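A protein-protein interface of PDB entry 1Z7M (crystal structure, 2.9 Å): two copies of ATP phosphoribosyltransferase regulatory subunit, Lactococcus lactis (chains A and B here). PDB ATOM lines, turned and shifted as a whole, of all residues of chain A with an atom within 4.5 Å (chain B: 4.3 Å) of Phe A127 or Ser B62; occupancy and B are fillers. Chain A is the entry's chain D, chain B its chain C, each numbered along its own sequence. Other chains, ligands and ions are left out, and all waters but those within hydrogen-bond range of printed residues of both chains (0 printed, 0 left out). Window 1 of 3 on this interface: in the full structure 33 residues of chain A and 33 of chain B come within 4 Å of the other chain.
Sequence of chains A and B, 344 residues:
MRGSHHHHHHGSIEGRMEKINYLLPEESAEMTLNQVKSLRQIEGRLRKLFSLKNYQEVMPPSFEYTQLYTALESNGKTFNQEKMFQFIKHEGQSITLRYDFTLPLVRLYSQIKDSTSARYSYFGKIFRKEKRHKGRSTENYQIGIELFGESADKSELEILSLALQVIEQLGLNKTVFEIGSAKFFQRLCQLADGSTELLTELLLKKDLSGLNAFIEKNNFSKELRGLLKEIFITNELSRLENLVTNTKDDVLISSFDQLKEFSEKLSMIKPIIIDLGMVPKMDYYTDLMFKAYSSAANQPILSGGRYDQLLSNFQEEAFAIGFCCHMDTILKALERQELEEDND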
ATOM      1  N   LYS A  83     -25.096   8.467  35.696  1.00  0.00           N
ATOM      2  CA  LYS A  83     -23.828   7.750  35.640  1.00  0.00           C
ATOM      3  C   LYS A  83     -23.430   7.325  34.233  1.00  0.00           C
ATOM      4  O   LYS A  83     -22.412   6.661  34.053  1.00  0.00           O
ATOM      5  CB  LYS A  83     -23.875   6.519  36.540  1.00  0.00           C
ATOM      6  CG  LYS A  83     -23.952   6.836  38.014  1.00  0.00           C
ATOM      7  CD  LYS A  83     -24.158   5.562  38.822  1.00  0.00           C
ATOM      8  CE  LYS A  83     -24.265   5.847  40.314  1.00  0.00           C
ATOM      9  NZ  LYS A  83     -22.990   6.397  40.867  1.00  0.00           N
ATOM     10  N   PHE A  85     -22.347   8.029  30.187  1.00  0.00           N
ATOM     11  CA  PHE A  85     -21.681   8.937  29.274  1.00  0.00           C
ATOM     12  C   PHE A  85     -22.535   8.945  28.015  1.00  0.00           C
ATOM     13  O   PHE A  85     -22.800   7.897  27.422  1.00  0.00           O
ATOM     14  CB  PHE A  85     -20.278   8.451  28.951  1.00  0.00           C
ATOM     15  CG  PHE A  85     -19.342   8.493  30.112  1.00  0.00           C
ATOM     16  CD1 PHE A  85     -19.233   7.414  30.971  1.00  0.00           C
ATOM     17  CD2 PHE A  85     -18.526   9.593  30.317  1.00  0.00           C
ATOM     18  CE1 PHE A  85     -18.310   7.424  32.019  1.00  0.00           C
ATOM     19  CE2 PHE A  85     -17.600   9.616  31.361  1.00  0.00           C
ATOM     20  CZ  PHE A  85     -17.491   8.526  32.213  1.00  0.00           C
ATOM     21  N   LEU A  97     -22.465   5.224  26.064  1.00  0.00           N
ATOM     22  CA  LEU A  97     -21.364   4.260  26.095  1.00  0.00           C
ATOM     23  C   LEU A  97     -21.809   2.981  26.807  1.00  0.00           C
ATOM     24  O   LEU A  97     -22.600   3.048  27.750  1.00  0.00           O
ATOM     25  CB  LEU A  97     -20.176   4.814  26.872  1.00  0.00           C
ATOM     26  CG  LEU A  97     -19.051   5.507  26.136  1.00  0.00           C
ATOM     27  CD1 LEU A  97     -17.928   5.661  27.094  1.00  0.00           C
ATOM     28  CD2 LEU A  97     -18.574   4.695  24.969  1.00  0.00           C
ATOM     29  N   ARG A  98     -21.285   1.831  26.377  1.00  0.00           N
ATOM     30  CA  ARG A  98     -21.646   0.559  26.995  1.00  0.00           C
ATOM     31  C   ARG A  98     -21.682   0.778  28.485  1.00  0.00           C
ATOM     32  O   ARG A  98     -20.699   1.216  29.085  1.00  0.00           O
ATOM     33  CB  ARG A  98     -20.624  -0.518  26.675  1.00  0.00           C
ATOM     34  CG  ARG A  98     -21.218  -1.759  26.070  1.00  0.00           C
ATOM     35  CD  ARG A  98     -20.514  -2.990  26.600  1.00  0.00           C
ATOM     36  NE  ARG A  98     -19.078  -2.809  26.844  1.00  0.00           N
ATOM     37  CZ  ARG A  98     -18.151  -2.640  25.905  1.00  0.00           C
ATOM     38  NH1 ARG A  98     -18.478  -2.614  24.617  1.00  0.00           N
ATOM     39  NH2 ARG A  98     -16.882  -2.520  26.265  1.00  0.00           N
ATOM     40  N   TYR A  99     -22.823   0.473  29.081  1.00  0.00           N
ATOM     41  CA  TYR A  99     -23.023   0.673  30.507  1.00  0.00           C
ATOM     42  C   TYR A  99     -23.276  -0.655  31.211  1.00  0.00           C
ATOM     43  O   TYR A  99     -23.065  -0.783  32.417  1.00  0.00           O
ATOM     44  CB  TYR A  99     -24.227   1.607  30.707  1.00  0.00           C
ATOM     45  CG  TYR A  99     -24.519   1.988  32.137  1.00  0.00           C
ATOM     46  CD1 TYR A  99     -23.628   2.769  32.863  1.00  0.00           C
ATOM     47  CD2 TYR A  99     -25.686   1.560  32.763  1.00  0.00           C
ATOM     48  CE1 TYR A  99     -23.886   3.114  34.170  1.00  0.00           C
ATOM     49  CE2 TYR A  99     -25.952   1.899  34.069  1.00  0.00           C
ATOM     50  CZ  TYR A  99     -25.047   2.676  34.769  1.00  0.00           C
ATOM     51  OH  TYR A  99     -25.298   2.994  36.084  1.00  0.00           O
ATOM     52  N   LYS A 125     -15.075  -3.898  29.101  1.00  0.00           N
ATOM     53  CA  LYS A 125     -15.427  -2.942  30.120  1.00  0.00           C
ATOM     54  C   LYS A 125     -16.687  -2.118  29.842  1.00  0.00           C
ATOM     55  O   LYS A 125     -17.115  -1.963  28.694  1.00  0.00           O
ATOM     56  CB  LYS A 125     -14.210  -2.037  30.385  1.00  0.00           C
ATOM     57  CG  LYS A 125     -13.864  -1.068  29.281  1.00  0.00           C
ATOM     58  CD  LYS A 125     -12.346  -0.888  29.062  1.00  0.00           C
ATOM     59  CE  LYS A 125     -11.547  -0.430  30.261  1.00  0.00           C
ATOM     60  NZ  LYS A 125     -10.151  -0.070  29.871  1.00  0.00           N
ATOM     61  N   ILE A 126     -17.287  -1.630  30.930  1.00  0.00           N
ATOM     62  CA  ILE A 126     -18.478  -0.776  30.897  1.00  0.00           C
ATOM     63  C   ILE A 126     -18.051   0.597  31.435  1.00  0.00           C
ATOM     64  O   ILE A 126     -17.063   0.702  32.173  1.00  0.00           O
ATOM     65  CB  ILE A 126     -19.605  -1.324  31.794  1.00  0.00           C
ATOM     66  CG1 ILE A 126     -19.112  -1.411  33.232  1.00  0.00           C
ATOM     67  CG2 ILE A 126     -20.052  -2.679  31.305  1.00  0.00           C
ATOM     68  CD1 ILE A 126     -20.166  -1.851  34.195  1.00  0.00           C
ATOM     69  N   PHE A 127     -18.789   1.643  31.077  1.00  0.00           N
ATOM     70  CA  PHE A 127     -18.424   2.991  31.512  1.00  0.00           C
ATOM     71  C   PHE A 127     -19.480   3.734  32.336  1.00  0.00           C
ATOM     72  O   PHE A 127     -20.565   4.052  31.844  1.00  0.00           O
ATOM     73  CB  PHE A 127     -18.030   3.834  30.291  1.00  0.00           C
ATOM     74  CG  PHE A 127     -17.122   3.118  29.330  1.00  0.00           C
ATOM     75  CD1 PHE A 127     -17.652   2.316  28.316  1.00  0.00           C
ATOM     76  CD2 PHE A 127     -15.735   3.204  29.464  1.00  0.00           C
ATOM     77  CE1 PHE A 127     -16.816   1.609  27.454  1.00  0.00           C
ATOM     78  CE2 PHE A 127     -14.898   2.504  28.610  1.00  0.00           C
ATOM     79  CZ  PHE A 127     -15.439   1.703  27.604  1.00  0.00           C
ATOM     80  N   ARG A 128     -19.134   4.017  33.591  1.00  0.00           N
ATOM     81  CA  ARG A 128     -20.020   4.719  34.518  1.00  0.00           C
ATOM     82  C   ARG A 128     -19.286   5.910  35.121  1.00  0.00           C
ATOM     83  O   ARG A 128     -18.058   5.935  35.152  1.00  0.00           O
ATOM     84  CB  ARG A 128     -20.449   3.786  35.646  1.00  0.00           C
ATOM     85  CG  ARG A 128     -20.927   2.426  35.181  1.00  0.00           C
ATOM     86  CD  ARG A 128     -20.852   1.399  36.315  1.00  0.00           C
ATOM     87  NE  ARG A 128     -22.138   1.196  36.979  1.00  0.00           N
ATOM     88  CZ  ARG A 128     -23.095   0.375  36.547  1.00  0.00           C
ATOM     89  NH1 ARG A 128     -22.929  -0.340  35.437  1.00  0.00           N
ATOM     90  NH2 ARG A 128     -24.229   0.274  37.237  1.00  0.00           N
ATOM     91  N   THR A 138     -13.634   4.616  37.001  1.00  0.00           N
ATOM     92  CA  THR A 138     -14.617   5.018  36.013  1.00  0.00           C
ATOM     93  C   THR A 138     -14.740   3.901  34.982  1.00  0.00           C
ATOM     94  O   THR A 138     -15.844   3.564  34.541  1.00  0.00           O
ATOM     95  CB  THR A 138     -14.193   6.292  35.305  1.00  0.00           C
ATOM     96  OG1 THR A 138     -13.864   7.277  36.288  1.00  0.00           O
ATOM     97  CG2 THR A 138     -15.324   6.807  34.419  1.00  0.00           C
ATOM     98  N   GLU A 139     -13.598   3.334  34.596  1.00  0.00           N
ATOM     99  CA  GLU A 139     -13.582   2.245  33.626  1.00  0.00           C
ATOM    100  C   GLU A 139     -13.538   0.931  34.367  1.00  0.00           C
ATOM    101  O   GLU A 139     -12.610   0.639  35.119  1.00  0.00           O
ATOM    102  CB  GLU A 139     -12.391   2.362  32.696  1.00  0.00           C
ATOM    103  CG  GLU A 139     -12.374   3.638  31.915  1.00  0.00           C
ATOM    104  CD  GLU A 139     -11.237   3.663  30.945  1.00  0.00           C
ATOM    105  OE1 GLU A 139     -10.562   4.708  30.834  1.00  0.00           O
ATOM    106  OE2 GLU A 139     -11.016   2.623  30.295  1.00  0.00           O
ATOM    107  N   PRO B  60      -4.279   1.763  26.914  1.00  0.00           N
ATOM    108  CA  PRO B  60      -4.495   3.208  27.058  1.00  0.00           C
ATOM    109  C   PRO B  60      -5.865   3.535  27.637  1.00  0.00           C
ATOM    110  O   PRO B  60      -6.833   2.813  27.414  1.00  0.00           O
ATOM    111  CB  PRO B  60      -4.367   3.725  25.624  1.00  0.00           C
ATOM    112  CG  PRO B  60      -3.605   2.643  24.910  1.00  0.00           C
ATOM    113  CD  PRO B  60      -4.162   1.396  25.493  1.00  0.00           C
ATOM    114  N   PRO B  61      -5.968   4.637  28.383  1.00  0.00           N
ATOM    115  CA  PRO B  61      -7.262   5.006  28.957  1.00  0.00           C
ATOM    116  C   PRO B  61      -8.295   5.195  27.850  1.00  0.00           C
ATOM    117  O   PRO B  61      -7.940   5.478  26.704  1.00  0.00           O
ATOM    118  CB  PRO B  61      -6.955   6.313  29.676  1.00  0.00           C
ATOM    119  CG  PRO B  61      -5.837   6.888  28.856  1.00  0.00           C
ATOM    120  CD  PRO B  61      -4.968   5.680  28.642  1.00  0.00           C
ATOM    121  N   SER B  62      -9.570   5.045  28.190  1.00  0.00           N
ATOM    122  CA  SER B  62     -10.646   5.210  27.219  1.00  0.00           C
ATOM    123  C   SER B  62     -11.046   6.689  27.084  1.00  0.00           C
ATOM    124  O   SER B  62     -11.729   7.079  26.129  1.00  0.00           O
ATOM    125  CB  SER B  62     -11.848   4.364  27.642  1.00  0.00           C
ATOM    126  OG  SER B  62     -11.480   3.002  27.746  1.00  0.00           O
ATOM    127  N   PHE B  63     -10.618   7.501  28.050  1.00  0.00           N
ATOM    128  CA  PHE B  63     -10.914   8.930  28.046  1.00  0.00           C
ATOM    129  C   PHE B  63      -9.634   9.732  27.980  1.00  0.00           C
ATOM    130  O   PHE B  63      -8.657   9.406  28.643  1.00  0.00           O
ATOM    131  CB  PHE B  63     -11.713   9.328  29.291  1.00  0.00           C
ATOM    132  CG  PHE B  63     -13.025   8.608  29.409  1.00  0.00           C
ATOM    133  CD1 PHE B  63     -13.146   7.485  30.218  1.00  0.00           C
ATOM    134  CD2 PHE B  63     -14.118   8.994  28.633  1.00  0.00           C
ATOM    135  CE1 PHE B  63     -14.333   6.751  30.250  1.00  0.00           C
ATOM    136  CE2 PHE B  63     -15.305   8.267  28.658  1.00  0.00           C
ATOM    137  CZ  PHE B  63     -15.412   7.141  29.468  1.00  0.00           C
ATOM    138  N   THR B  96     -12.440  13.403  25.258  1.00  0.00           N
ATOM    139  CA  THR B  96     -12.757  12.625  24.055  1.00  0.00           C
ATOM    140  C   THR B  96     -12.472  11.129  24.231  1.00  0.00           C
ATOM    141  O   THR B  96     -11.443  10.758  24.790  1.00  0.00           O
ATOM    142  CB  THR B  96     -11.924  13.118  22.866  1.00  0.00           C
ATOM    143  OG1 THR B  96     -12.117  14.525  22.703  1.00  0.00           O
ATOM    144  CG2 THR B  96     -12.328  12.401  21.596  1.00  0.00           C
ATOM    145  N   LEU B  97     -13.384  10.276  23.764  1.00  0.00           N
ATOM    146  CA  LEU B  97     -13.190   8.833  23.854  1.00  0.00           C
ATOM    147  C   LEU B  97     -11.948   8.520  23.024  1.00  0.00           C
ATOM    148  O   LEU B  97     -11.676   9.206  22.040  1.00  0.00           O
ATOM    149  CB  LEU B  97     -14.394   8.087  23.272  1.00  0.00           C
ATOM    150  CG  LEU B  97     -15.765   8.325  23.904  1.00  0.00           C
ATOM    151  CD1 LEU B  97     -16.762   7.270  23.421  1.00  0.00           C
ATOM    152  CD2 LEU B  97     -15.633   8.251  25.395  1.00  0.00           C
ATOM    153  N   ARG B  98     -11.196   7.496  23.425  1.00  0.00           N
ATOM    154  CA  ARG B  98      -9.972   7.091  22.722  1.00  0.00           C
ATOM    155  C   ARG B  98     -10.150   7.128  21.201  1.00  0.00           C
ATOM    156  O   ARG B  98     -10.870   6.312  20.615  1.00  0.00           O
ATOM    157  CB  ARG B  98      -9.562   5.691  23.173  1.00  0.00           C
ATOM    158  CG  ARG B  98      -8.151   5.350  22.814  1.00  0.00           C
ATOM    159  CD  ARG B  98      -7.756   4.040  23.413  1.00  0.00           C
ATOM    160  NE  ARG B  98      -8.652   2.971  23.009  1.00  0.00           N
ATOM    161  CZ  ARG B  98      -9.278   2.169  23.863  1.00  0.00           C
ATOM    162  NH1 ARG B  98      -9.101   2.330  25.162  1.00  0.00           N
ATOM    163  NH2 ARG B  98     -10.070   1.203  23.420  1.00  0.00           N
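OG of Ser B62 is in hydrogen-bond range of OE2 of Glu A139 (2.6 Å).
The backbone NH (N) of Arg B98 sits at hydrogen-bond distance from the backbone carbonyl oxygen (O) of Ser B62, 2.8 Å away. The backbone carbonyl oxygen (O) of Phe A85 is in hydrogen-bond range of the backbone NH (N) of Leu A97 (3.0 Å). The backbone carbonyl oxygen of Lys A125 sits at hydrogen-bond distance from the guanidinium group of Arg A98, 2.5 Å away. The backbone carbonyl oxygen (O) of Arg A98 sits at hydrogen-bond distance from the backbone NH (N) of Phe A127 (2.8 Å). The side-chain amino group of Lys A125 lies within salt-bridge range of the side-chain carboxylate of Glu A139, 2.9 Å away.
Among the printed residues, pairs that only touch across the chains: Phe A85 with Phe B63 (3.7 Å), Leu A97 with Phe B63 (3.8 Å), Leu A97 with Leu B97 (3.5 Å), Lys A125 with Ser B62 (3.96 Å), Phe A127 with Ser B62 (3.6 Å), Phe A127 with Phe B63 (3.9 Å), Glu A139 with Pro B61 (3.8 Å) and Glu A139 with Phe B63 (3.8 Å).
Phe A127 touches two residues of chain B. Of chain A, only Lys A125, Phe A127 and Glu A139 come within 4 Å of Ser B62. Printed residues of chain A within 4 Å of Phe B63: Phe A85 (3.7 Å), Leu A97 (3.8 Å), Phe A127 (3.9 Å) and Glu A139 (3.8 Å). Printed residues of chain A within 4 Å of Leu B97: Leu A97 (3.5 Å). Of the printed residues of chain B, Phe A85 touches Phe B63 (3.7 Å). Printed residues of chain A within 4 Å of Pro B61: Glu A139. Printed residues of chain B within 4 Å of Lys A125: Ser B62 (3.96 Å).
Of the 11 printed residues of chain A, 5 touch a printed residue of chain B. Printed residues of chain A that touch a printed residue of chain B: Phe A85, Leu A97, Lys A125, Phe A127 and Glu A139. Hydrophobic or aromatic side chains of chain A that line the printed part of chain B: Phe A85, Leu A97 and Phe A127. Of the 7 printed residues of chain B, 4 touch a printed residue of chain A. Printed residues of chain B that touch a printed residue of chain A: Pro B61, Ser B62, Phe B63 and Leu B97. Hydrophobic or aromatic side chains of chain B within 4 Å of the printed part of chain A: Phe B63 and Leu B97. Along chain B the printed residues that touch a printed residue of chain A span positions 61 to 97. Among the printed residues, 9 pairs touch across the chains. Among the printed residues, no Asp or Glu carboxylate lies within 4 Å of a Lys or Arg side-chain nitrogen of the other chain.
Leu A97 touches its own counterpart, Leu B97. Positions printed for both chains: 97 and 98.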
